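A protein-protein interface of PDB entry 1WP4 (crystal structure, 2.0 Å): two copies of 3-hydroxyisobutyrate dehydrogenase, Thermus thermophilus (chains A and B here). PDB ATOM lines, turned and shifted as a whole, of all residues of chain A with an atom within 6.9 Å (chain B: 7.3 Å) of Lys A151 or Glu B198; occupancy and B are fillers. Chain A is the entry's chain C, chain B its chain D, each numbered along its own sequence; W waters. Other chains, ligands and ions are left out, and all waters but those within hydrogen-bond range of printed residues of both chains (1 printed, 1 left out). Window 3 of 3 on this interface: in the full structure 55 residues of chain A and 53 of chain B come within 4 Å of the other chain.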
ATOM      1  N   GLY A 126     -28.892  18.745 -28.418  1.00  0.00           N
ATOM      2  CA  GLY A 126     -28.637  17.889 -27.272  1.00  0.00           C
ATOM      3  C   GLY A 126     -27.286  17.202 -27.386  1.00  0.00           C
ATOM      4  O   GLY A 126     -27.095  16.080 -26.901  1.00  0.00           O
ATOM      5  N   THR A 127     -26.334  17.878 -28.019  1.00  0.00           N
ATOM      6  CA  THR A 127     -25.001  17.314 -28.203  1.00  0.00           C
ATOM      7  C   THR A 127     -23.909  18.173 -27.572  1.00  0.00           C
ATOM      8  O   THR A 127     -22.756  18.140 -28.006  1.00  0.00           O
ATOM      9  CB  THR A 127     -24.684  17.157 -29.701  1.00  0.00           C
ATOM     10  OG1 THR A 127     -24.690  18.449 -30.324  1.00  0.00           O
ATOM     11  CG2 THR A 127     -25.726  16.272 -30.379  1.00  0.00           C
ATOM     12  N   LEU A 128     -24.271  18.939 -26.548  1.00  0.00           N
ATOM     13  CA  LEU A 128     -23.308  19.802 -25.879  1.00  0.00           C
ATOM     14  C   LEU A 128     -22.168  19.031 -25.232  1.00  0.00           C
ATOM     15  O   LEU A 128     -22.337  17.901 -24.781  1.00  0.00           O
ATOM     16  CB  LEU A 128     -24.001  20.643 -24.803  1.00  0.00           C
ATOM     17  CG  LEU A 128     -25.025  21.691 -25.254  1.00  0.00           C
ATOM     18  CD1 LEU A 128     -25.742  22.245 -24.029  1.00  0.00           C
ATOM     19  CD2 LEU A 128     -24.322  22.811 -26.023  1.00  0.00           C
ATOM     20  N   THR A 129     -20.997  19.654 -25.206  1.00  0.00           N
ATOM     21  CA  THR A 129     -19.829  19.070 -24.563  1.00  0.00           C
ATOM     22  C   THR A 129     -19.860  19.625 -23.139  1.00  0.00           C
ATOM     23  O   THR A 129     -20.074  20.821 -22.935  1.00  0.00           O
ATOM     24  CB  THR A 129     -18.521  19.511 -25.260  1.00  0.00           C
ATOM     25  OG1 THR A 129     -18.436  18.897 -26.549  1.00  0.00           O
ATOM     26  CG2 THR A 129     -17.307  19.118 -24.431  1.00  0.00           C
ATOM     27  N   VAL A 130     -19.672  18.759 -22.153  1.00  0.00           N
ATOM     28  CA  VAL A 130     -19.691  19.195 -20.762  1.00  0.00           C
ATOM     29  C   VAL A 130     -18.359  18.931 -20.067  1.00  0.00           C
ATOM     30  O   VAL A 130     -17.792  17.845 -20.178  1.00  0.00           O
ATOM     31  CB  VAL A 130     -20.812  18.479 -19.966  1.00  0.00           C
ATOM     32  CG1 VAL A 130     -20.826  18.972 -18.524  1.00  0.00           C
ATOM     33  CG2 VAL A 130     -22.165  18.729 -20.619  1.00  0.00           C
ATOM     34  N   MET A 131     -17.856  19.940 -19.366  1.00  0.00           N
ATOM     35  CA  MET A 131     -16.611  19.810 -18.621  1.00  0.00           C
ATOM     36  C   MET A 131     -17.008  19.896 -17.152  1.00  0.00           C
ATOM     37  O   MET A 131     -17.365  20.963 -16.650  1.00  0.00           O
ATOM     38  CB  MET A 131     -15.628  20.921 -19.014  1.00  0.00           C
ATOM     39  CG  MET A 131     -16.230  22.318 -19.080  1.00  0.00           C
ATOM     40  SD  MET A 131     -15.621  23.234 -20.519  1.00  0.00           S
ATOM     41  CE  MET A 131     -16.748  22.641 -21.776  1.00  0.00           C
ATOM     42  N   ARG A 143     -24.082  11.883 -14.505  1.00  0.00           N
ATOM     43  CA  ARG A 143     -23.970  11.595 -15.936  1.00  0.00           C
ATOM     44  C   ARG A 143     -25.278  11.238 -16.644  1.00  0.00           C
ATOM     45  O   ARG A 143     -25.591  11.802 -17.692  1.00  0.00           O
ATOM     46  CB  ARG A 143     -22.949  10.474 -16.190  1.00  0.00           C
ATOM     47  CG  ARG A 143     -21.496  10.929 -16.218  1.00  0.00           C
ATOM     48  CD  ARG A 143     -20.547   9.748 -16.468  1.00  0.00           C
ATOM     49  NE  ARG A 143     -19.139  10.133 -16.365  1.00  0.00           N
ATOM     50  CZ  ARG A 143     -18.457  10.777 -17.307  1.00  0.00           C
ATOM     51  NH1 ARG A 143     -19.043  11.117 -18.449  1.00  0.00           N
ATOM     52  NH2 ARG A 143     -17.185  11.097 -17.101  1.00  0.00           N
ATOM     53  N   ALA A 149     -26.428  16.643 -23.371  1.00  0.00           N
ATOM     54  CA  ALA A 149     -25.024  16.501 -23.730  1.00  0.00           C
ATOM     55  C   ALA A 149     -24.632  15.226 -24.465  1.00  0.00           C
ATOM     56  O   ALA A 149     -25.374  14.245 -24.496  1.00  0.00           O
ATOM     57  CB  ALA A 149     -24.170  16.636 -22.471  1.00  0.00           C
ATOM     58  N   LYS A 150     -23.447  15.262 -25.063  1.00  0.00           N
ATOM     59  CA  LYS A 150     -22.904  14.110 -25.772  1.00  0.00           C
ATOM     60  C   LYS A 150     -21.571  13.779 -25.109  1.00  0.00           C
ATOM     61  O   LYS A 150     -21.449  12.790 -24.391  1.00  0.00           O
ATOM     62  CB  LYS A 150     -22.689  14.430 -27.251  1.00  0.00           C
ATOM     63  CG  LYS A 150     -22.181  13.244 -28.057  1.00  0.00           C
ATOM     64  CD  LYS A 150     -22.076  13.572 -29.538  1.00  0.00           C
ATOM     65  CE  LYS A 150     -21.599  12.364 -30.328  1.00  0.00           C
ATOM     66  NZ  LYS A 150     -21.471  12.668 -31.781  1.00  0.00           N
ATOM     67  N   LYS A 151     -20.579  14.630 -25.339  1.00  0.00           N
ATOM     68  CA  LYS A 151     -19.249  14.455 -24.766  1.00  0.00           C
ATOM     69  C   LYS A 151     -19.227  15.056 -23.361  1.00  0.00           C
ATOM     70  O   LYS A 151     -19.467  16.251 -23.190  1.00  0.00           O
ATOM     71  CB  LYS A 151     -18.213  15.164 -25.643  1.00  0.00           C
ATOM     72  CG  LYS A 151     -16.763  15.017 -25.184  1.00  0.00           C
ATOM     73  CD  LYS A 151     -16.216  13.628 -25.473  1.00  0.00           C
ATOM     74  CE  LYS A 151     -14.719  13.567 -25.216  1.00  0.00           C
ATOM     75  NZ  LYS A 151     -14.145  12.255 -25.613  1.00  0.00           N
ATOM     76  N   VAL A 152     -18.949  14.220 -22.363  1.00  0.00           N
ATOM     77  CA  VAL A 152     -18.889  14.654 -20.972  1.00  0.00           C
ATOM     78  C   VAL A 152     -17.539  14.241 -20.395  1.00  0.00           C
ATOM     79  O   VAL A 152     -17.231  13.054 -20.313  1.00  0.00           O
ATOM     80  CB  VAL A 152     -20.014  14.010 -20.137  1.00  0.00           C
ATOM     81  CG1 VAL A 152     -19.911  14.462 -18.691  1.00  0.00           C
ATOM     82  CG2 VAL A 152     -21.373  14.384 -20.719  1.00  0.00           C
ATOM     83  N   VAL A 153     -16.740  15.228 -19.999  1.00  0.00           N
ATOM     84  CA  VAL A 153     -15.408  14.976 -19.465  1.00  0.00           C
ATOM     85  C   VAL A 153     -15.226  15.529 -18.056  1.00  0.00           C
ATOM     86  O   VAL A 153     -15.504  16.701 -17.791  1.00  0.00           O
ATOM     87  CB  VAL A 153     -14.324  15.609 -20.372  1.00  0.00           C
ATOM     88  CG1 VAL A 153     -12.933  15.189 -19.904  1.00  0.00           C
ATOM     89  CG2 VAL A 153     -14.554  15.201 -21.821  1.00  0.00           C
ATOM     90  N   HIS A 154     -14.763  14.668 -17.155  1.00  0.00           N
ATOM     91  CA  HIS A 154     -14.513  15.053 -15.772  1.00  0.00           C
ATOM     92  C   HIS A 154     -13.097  15.618 -15.767  1.00  0.00           C
ATOM     93  O   HIS A 154     -12.130  14.868 -15.911  1.00  0.00           O
ATOM     94  CB  HIS A 154     -14.593  13.825 -14.864  1.00  0.00           C
ATOM     95  CG  HIS A 154     -14.437  14.141 -13.410  1.00  0.00           C
ATOM     96  ND1 HIS A 154     -14.220  13.169 -12.457  1.00  0.00           N
ATOM     97  CD2 HIS A 154     -14.481  15.319 -12.744  1.00  0.00           C
ATOM     98  CE1 HIS A 154     -14.136  13.734 -11.266  1.00  0.00           C
ATOM     99  NE2 HIS A 154     -14.291  15.038 -11.412  1.00  0.00           N
ATOM    100  N   SER B 192      -5.072  18.281 -16.028  1.00  0.00           N
ATOM    101  CA  SER B 192      -4.344  17.515 -17.029  1.00  0.00           C
ATOM    102  C   SER B 192      -4.429  18.187 -18.398  1.00  0.00           C
ATOM    103  O   SER B 192      -5.512  18.576 -18.835  1.00  0.00           O
ATOM    104  CB  SER B 192      -4.929  16.105 -17.117  1.00  0.00           C
ATOM    105  OG  SER B 192      -4.569  15.481 -18.332  1.00  0.00           O
ATOM    106  N   ALA B 193      -3.290  18.326 -19.069  1.00  0.00           N
ATOM    107  CA  ALA B 193      -3.277  18.931 -20.394  1.00  0.00           C
ATOM    108  C   ALA B 193      -4.033  18.000 -21.334  1.00  0.00           C
ATOM    109  O   ALA B 193      -4.650  18.438 -22.303  1.00  0.00           O
ATOM    110  CB  ALA B 193      -1.847  19.120 -20.881  1.00  0.00           C
ATOM    111  N   GLU B 194      -3.985  16.707 -21.030  1.00  0.00           N
ATOM    112  CA  GLU B 194      -4.668  15.708 -21.840  1.00  0.00           C
ATOM    113  C   GLU B 194      -6.178  15.854 -21.666  1.00  0.00           C
ATOM    114  O   GLU B 194      -6.937  15.762 -22.633  1.00  0.00           O
ATOM    115  CB  GLU B 194      -4.220  14.305 -21.424  1.00  0.00           C
ATOM    116  CG  GLU B 194      -4.735  13.196 -22.316  1.00  0.00           C
ATOM    117  CD  GLU B 194      -4.234  11.830 -21.881  1.00  0.00           C
ATOM    118  OE1 GLU B 194      -3.000  11.643 -21.816  1.00  0.00           O
ATOM    119  OE2 GLU B 194      -5.074  10.946 -21.605  1.00  0.00           O
ATOM    120  N   LYS B 195      -6.609  16.080 -20.428  1.00  0.00           N
ATOM    121  CA  LYS B 195      -8.029  16.253 -20.132  1.00  0.00           C
ATOM    122  C   LYS B 195      -8.543  17.559 -20.737  1.00  0.00           C
ATOM    123  O   LYS B 195      -9.641  17.608 -21.291  1.00  0.00           O
ATOM    124  CB  LYS B 195      -8.260  16.273 -18.617  1.00  0.00           C
ATOM    125  CG  LYS B 195      -8.235  14.903 -17.945  1.00  0.00           C
ATOM    126  CD  LYS B 195      -9.473  14.093 -18.296  1.00  0.00           C
ATOM    127  CE  LYS B 195      -9.550  12.816 -17.472  1.00  0.00           C
ATOM    128  NZ  LYS B 195     -10.867  12.133 -17.624  1.00  0.00           N
ATOM    129  N   ALA B 196      -7.739  18.610 -20.627  1.00  0.00           N
ATOM    130  CA  ALA B 196      -8.102  19.926 -21.149  1.00  0.00           C
ATOM    131  C   ALA B 196      -8.304  19.892 -22.659  1.00  0.00           C
ATOM    132  O   ALA B 196      -9.267  20.456 -23.180  1.00  0.00           O
ATOM    133  CB  ALA B 196      -7.022  20.943 -20.788  1.00  0.00           C
ATOM    134  N   LEU B 197      -7.388  19.231 -23.359  1.00  0.00           N
ATOM    135  CA  LEU B 197      -7.469  19.118 -24.809  1.00  0.00           C
ATOM    136  C   LEU B 197      -8.630  18.238 -25.247  1.00  0.00           C
ATOM    137  O   LEU B 197      -9.228  18.470 -26.295  1.00  0.00           O
ATOM    138  CB  LEU B 197      -6.154  18.570 -25.365  1.00  0.00           C
ATOM    139  CG  LEU B 197      -5.033  19.610 -25.348  1.00  0.00           C
ATOM    140  CD1 LEU B 197      -3.689  18.949 -25.603  1.00  0.00           C
ATOM    141  CD2 LEU B 197      -5.335  20.672 -26.399  1.00  0.00           C
ATOM    142  N   GLU B 198      -8.952  17.223 -24.451  1.00  0.00           N
ATOM    143  CA  GLU B 198     -10.066  16.348 -24.791  1.00  0.00           C
ATOM    144  C   GLU B 198     -11.328  17.211 -24.868  1.00  0.00           C
ATOM    145  O   GLU B 198     -12.152  17.050 -25.766  1.00  0.00           O
ATOM    146  CB  GLU B 198     -10.246  15.266 -23.723  1.00  0.00           C
ATOM    147  CG  GLU B 198     -11.172  14.132 -24.150  1.00  0.00           C
ATOM    148  CD  GLU B 198     -11.535  13.214 -23.001  1.00  0.00           C
ATOM    149  OE1 GLU B 198     -10.704  13.050 -22.082  1.00  0.00           O
ATOM    150  OE2 GLU B 198     -12.648  12.647 -23.021  1.00  0.00           O
ATOM    151  N   VAL B 199     -11.474  18.132 -23.921  1.00  0.00           N
ATOM    152  CA  VAL B 199     -12.636  19.021 -23.902  1.00  0.00           C
ATOM    153  C   VAL B 199     -12.540  20.064 -25.007  1.00  0.00           C
ATOM    154  O   VAL B 199     -13.490  20.273 -25.769  1.00  0.00           O
ATOM    155  CB  VAL B 199     -12.761  19.768 -22.545  1.00  0.00           C
ATOM    156  CG1 VAL B 199     -13.806  20.886 -22.655  1.00  0.00           C
ATOM    157  CG2 VAL B 199     -13.153  18.786 -21.444  1.00  0.00           C
ATOM    158  N   ILE B 200     -11.389  20.724 -25.087  1.00  0.00           N
ATOM    159  CA  ILE B 200     -11.177  21.773 -26.087  1.00  0.00           C
ATOM    160  C   ILE B 200     -11.371  21.296 -27.525  1.00  0.00           C
ATOM    161  O   ILE B 200     -11.982  21.986 -28.342  1.00  0.00           O
ATOM    162  CB  ILE B 200      -9.767  22.388 -25.941  1.00  0.00           C
ATOM    163  CG1 ILE B 200      -9.675  23.149 -24.618  1.00  0.00           C
ATOM    164  CG2 ILE B 200      -9.466  23.314 -27.117  1.00  0.00           C
ATOM    165  CD1 ILE B 200      -8.282  23.657 -24.287  1.00  0.00           C
ATOM    166  N   ASN B 201     -10.859  20.111 -27.838  1.00  0.00           N
ATOM    167  CA  ASN B 201     -10.990  19.587 -29.191  1.00  0.00           C
ATOM    168  C   ASN B 201     -12.424  19.175 -29.524  1.00  0.00           C
ATOM    169  O   ASN B 201     -12.733  18.831 -30.667  1.00  0.00           O
ATOM    170  CB  ASN B 201     -10.002  18.439 -29.391  1.00  0.00           C
ATOM    171  CG  ASN B 201      -8.563  18.935 -29.508  1.00  0.00           C
ATOM    172  OD1 ASN B 201      -7.616  18.273 -29.076  1.00  0.00           O
ATOM    173  ND2 ASN B 201      -8.399  20.107 -30.100  1.00  0.00           N
ATOM    174  N   ALA B 202     -13.299  19.225 -28.522  1.00  0.00           N
ATOM    175  CA  ALA B 202     -14.714  18.909 -28.707  1.00  0.00           C
ATOM    176  C   ALA B 202     -15.503  20.181 -28.378  1.00  0.00           C
ATOM    177  O   ALA B 202     -16.714  20.138 -28.157  1.00  0.00           O
ATOM    178  CB  ALA B 202     -15.140  17.767 -27.772  1.00  0.00           C
ATOM    179  N   SER B 203     -14.798  21.310 -28.353  1.00  0.00           N
ATOM    180  CA  SER B 203     -15.413  22.594 -28.031  1.00  0.00           C
ATOM    181  C   SER B 203     -15.063  23.703 -29.027  1.00  0.00           C
ATOM    182  O   SER B 203     -14.335  23.472 -29.994  1.00  0.00           O
ATOM    183  CB  SER B 203     -15.017  23.009 -26.614  1.00  0.00           C
ATOM    184  OG  SER B 203     -15.480  22.049 -25.673  1.00  0.00           O
ATOM    185  N   THR B 210      -4.541  22.711 -31.589  1.00  0.00           N
ATOM    186  CA  THR B 210      -4.923  21.898 -30.434  1.00  0.00           C
ATOM    187  C   THR B 210      -5.297  20.471 -30.824  1.00  0.00           C
ATOM    188  O   THR B 210      -5.134  19.537 -30.030  1.00  0.00           O
ATOM    189  CB  THR B 210      -6.126  22.501 -29.680  1.00  0.00           C
ATOM    190  OG1 THR B 210      -7.291  22.450 -30.517  1.00  0.00           O
ATOM    191  CG2 THR B 210      -5.839  23.945 -29.285  1.00  0.00           C
ATOM    192  N   PRO B 215      -1.158  17.788 -29.076  1.00  0.00           N
ATOM    193  CA  PRO B 215      -1.237  16.436 -28.512  1.00  0.00           C
ATOM    194  C   PRO B 215      -0.136  15.507 -29.026  1.00  0.00           C
ATOM    195  O   PRO B 215       0.537  14.833 -28.247  1.00  0.00           O
ATOM    196  CB  PRO B 215      -2.621  15.957 -28.945  1.00  0.00           C
ATOM    197  CG  PRO B 215      -3.401  17.230 -29.078  1.00  0.00           C
ATOM    198  CD  PRO B 215      -2.412  18.137 -29.764  1.00  0.00           C
HETATM  199  O   HOH W   1     -15.647  11.001 -23.145  1.00  0.00           O
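Printed residues of chain B within 4 Å of Thr A129: Ala B202 and Ser B203. Of chain B, only Glu B198 (3.0 Å) comes within 4 Å of Lys A151. Of the printed residues of chain B, His A154 touches Lys B195. Ser B192 touches none of the printed residues of chain A. Of the printed residues of chain A, Val B199 touches Met A131 and Val A153. Printed residues of chain A within 4 Å of Ala B202: Thr A129. Printed residues of chain A within 4 Å of Ser B203: Thr A129. Thr B210 touches none of the printed residues of chain A. The nearest residue of chain B that does not touch Lys A151 is Ala B202 (4.1 Å). The nearest residue of chain A that does not touch Glu B198 is Val A152 (5.3 Å). The nearest printed residue of chain B that does not touch Val A153 is Ala B196 (6.3 Å).
N of Val A130 is in hydrogen-bond range of O of Lys A151, at 2.7 Å. The backbone carbonyl oxygen of Val A130 sits at hydrogen-bond distance from the backbone NH of Val A153. The side-chain hydroxyl (OG) of Ser B192 sits at hydrogen-bond distance from the backbone NH (N) of Lys B195 (3.0 Å). O of Val B199 lies within hydrogen-bond range of OG of Ser B203.
The backbone carbonyl oxygen (O) of Ala B202 lies within hydrogen-bond range of the side-chain hydroxyl (OG1) of Thr A129 (2.7 Å). The side-chain carboxylate (OE2) of Glu B198 lies within salt-bridge range of the side-chain amino group (NZ) of Lys A151 (3.0 Å). The side-chain amino group (NZ) of Lys B195 sits at hydrogen-bond distance from the backbone carbonyl oxygen (O) of His A154 (3.5 Å).
No position is printed for both chains.
Of the 13 printed residues of chain A, 5 touch a printed residue of chain B. Printed residues of chain A that touch a printed residue of chain B: Thr A129, Met A131, Lys A151, Val A153 and His A154. Hydrophobic or aromatic side chains of chain A within 4 Å of the printed part of chain B: Met A131 and Val A153. Hydrophobic or aromatic side chains of chain B that line the printed part of chain A: Val B199 and Ala B202. Along chain B the printed residues that touch a printed residue of chain A span positions 195 to 203.
Among the printed residues, merely in contact across the chains: Thr A129 with Ser B203 (3.7 Å), Met A131 with Val B199 (3.5 Å), Val A153 with Lys B195 (3.97 Å), Val A153 with Glu B198 (3.4 Å) and Val A153 with Val B199 (3.6 Å).
Water W1 lies within hydrogen-bond range of NZ of Lys A151 (3.1 Å) and OE2 of Glu B198 (3.4 Å).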
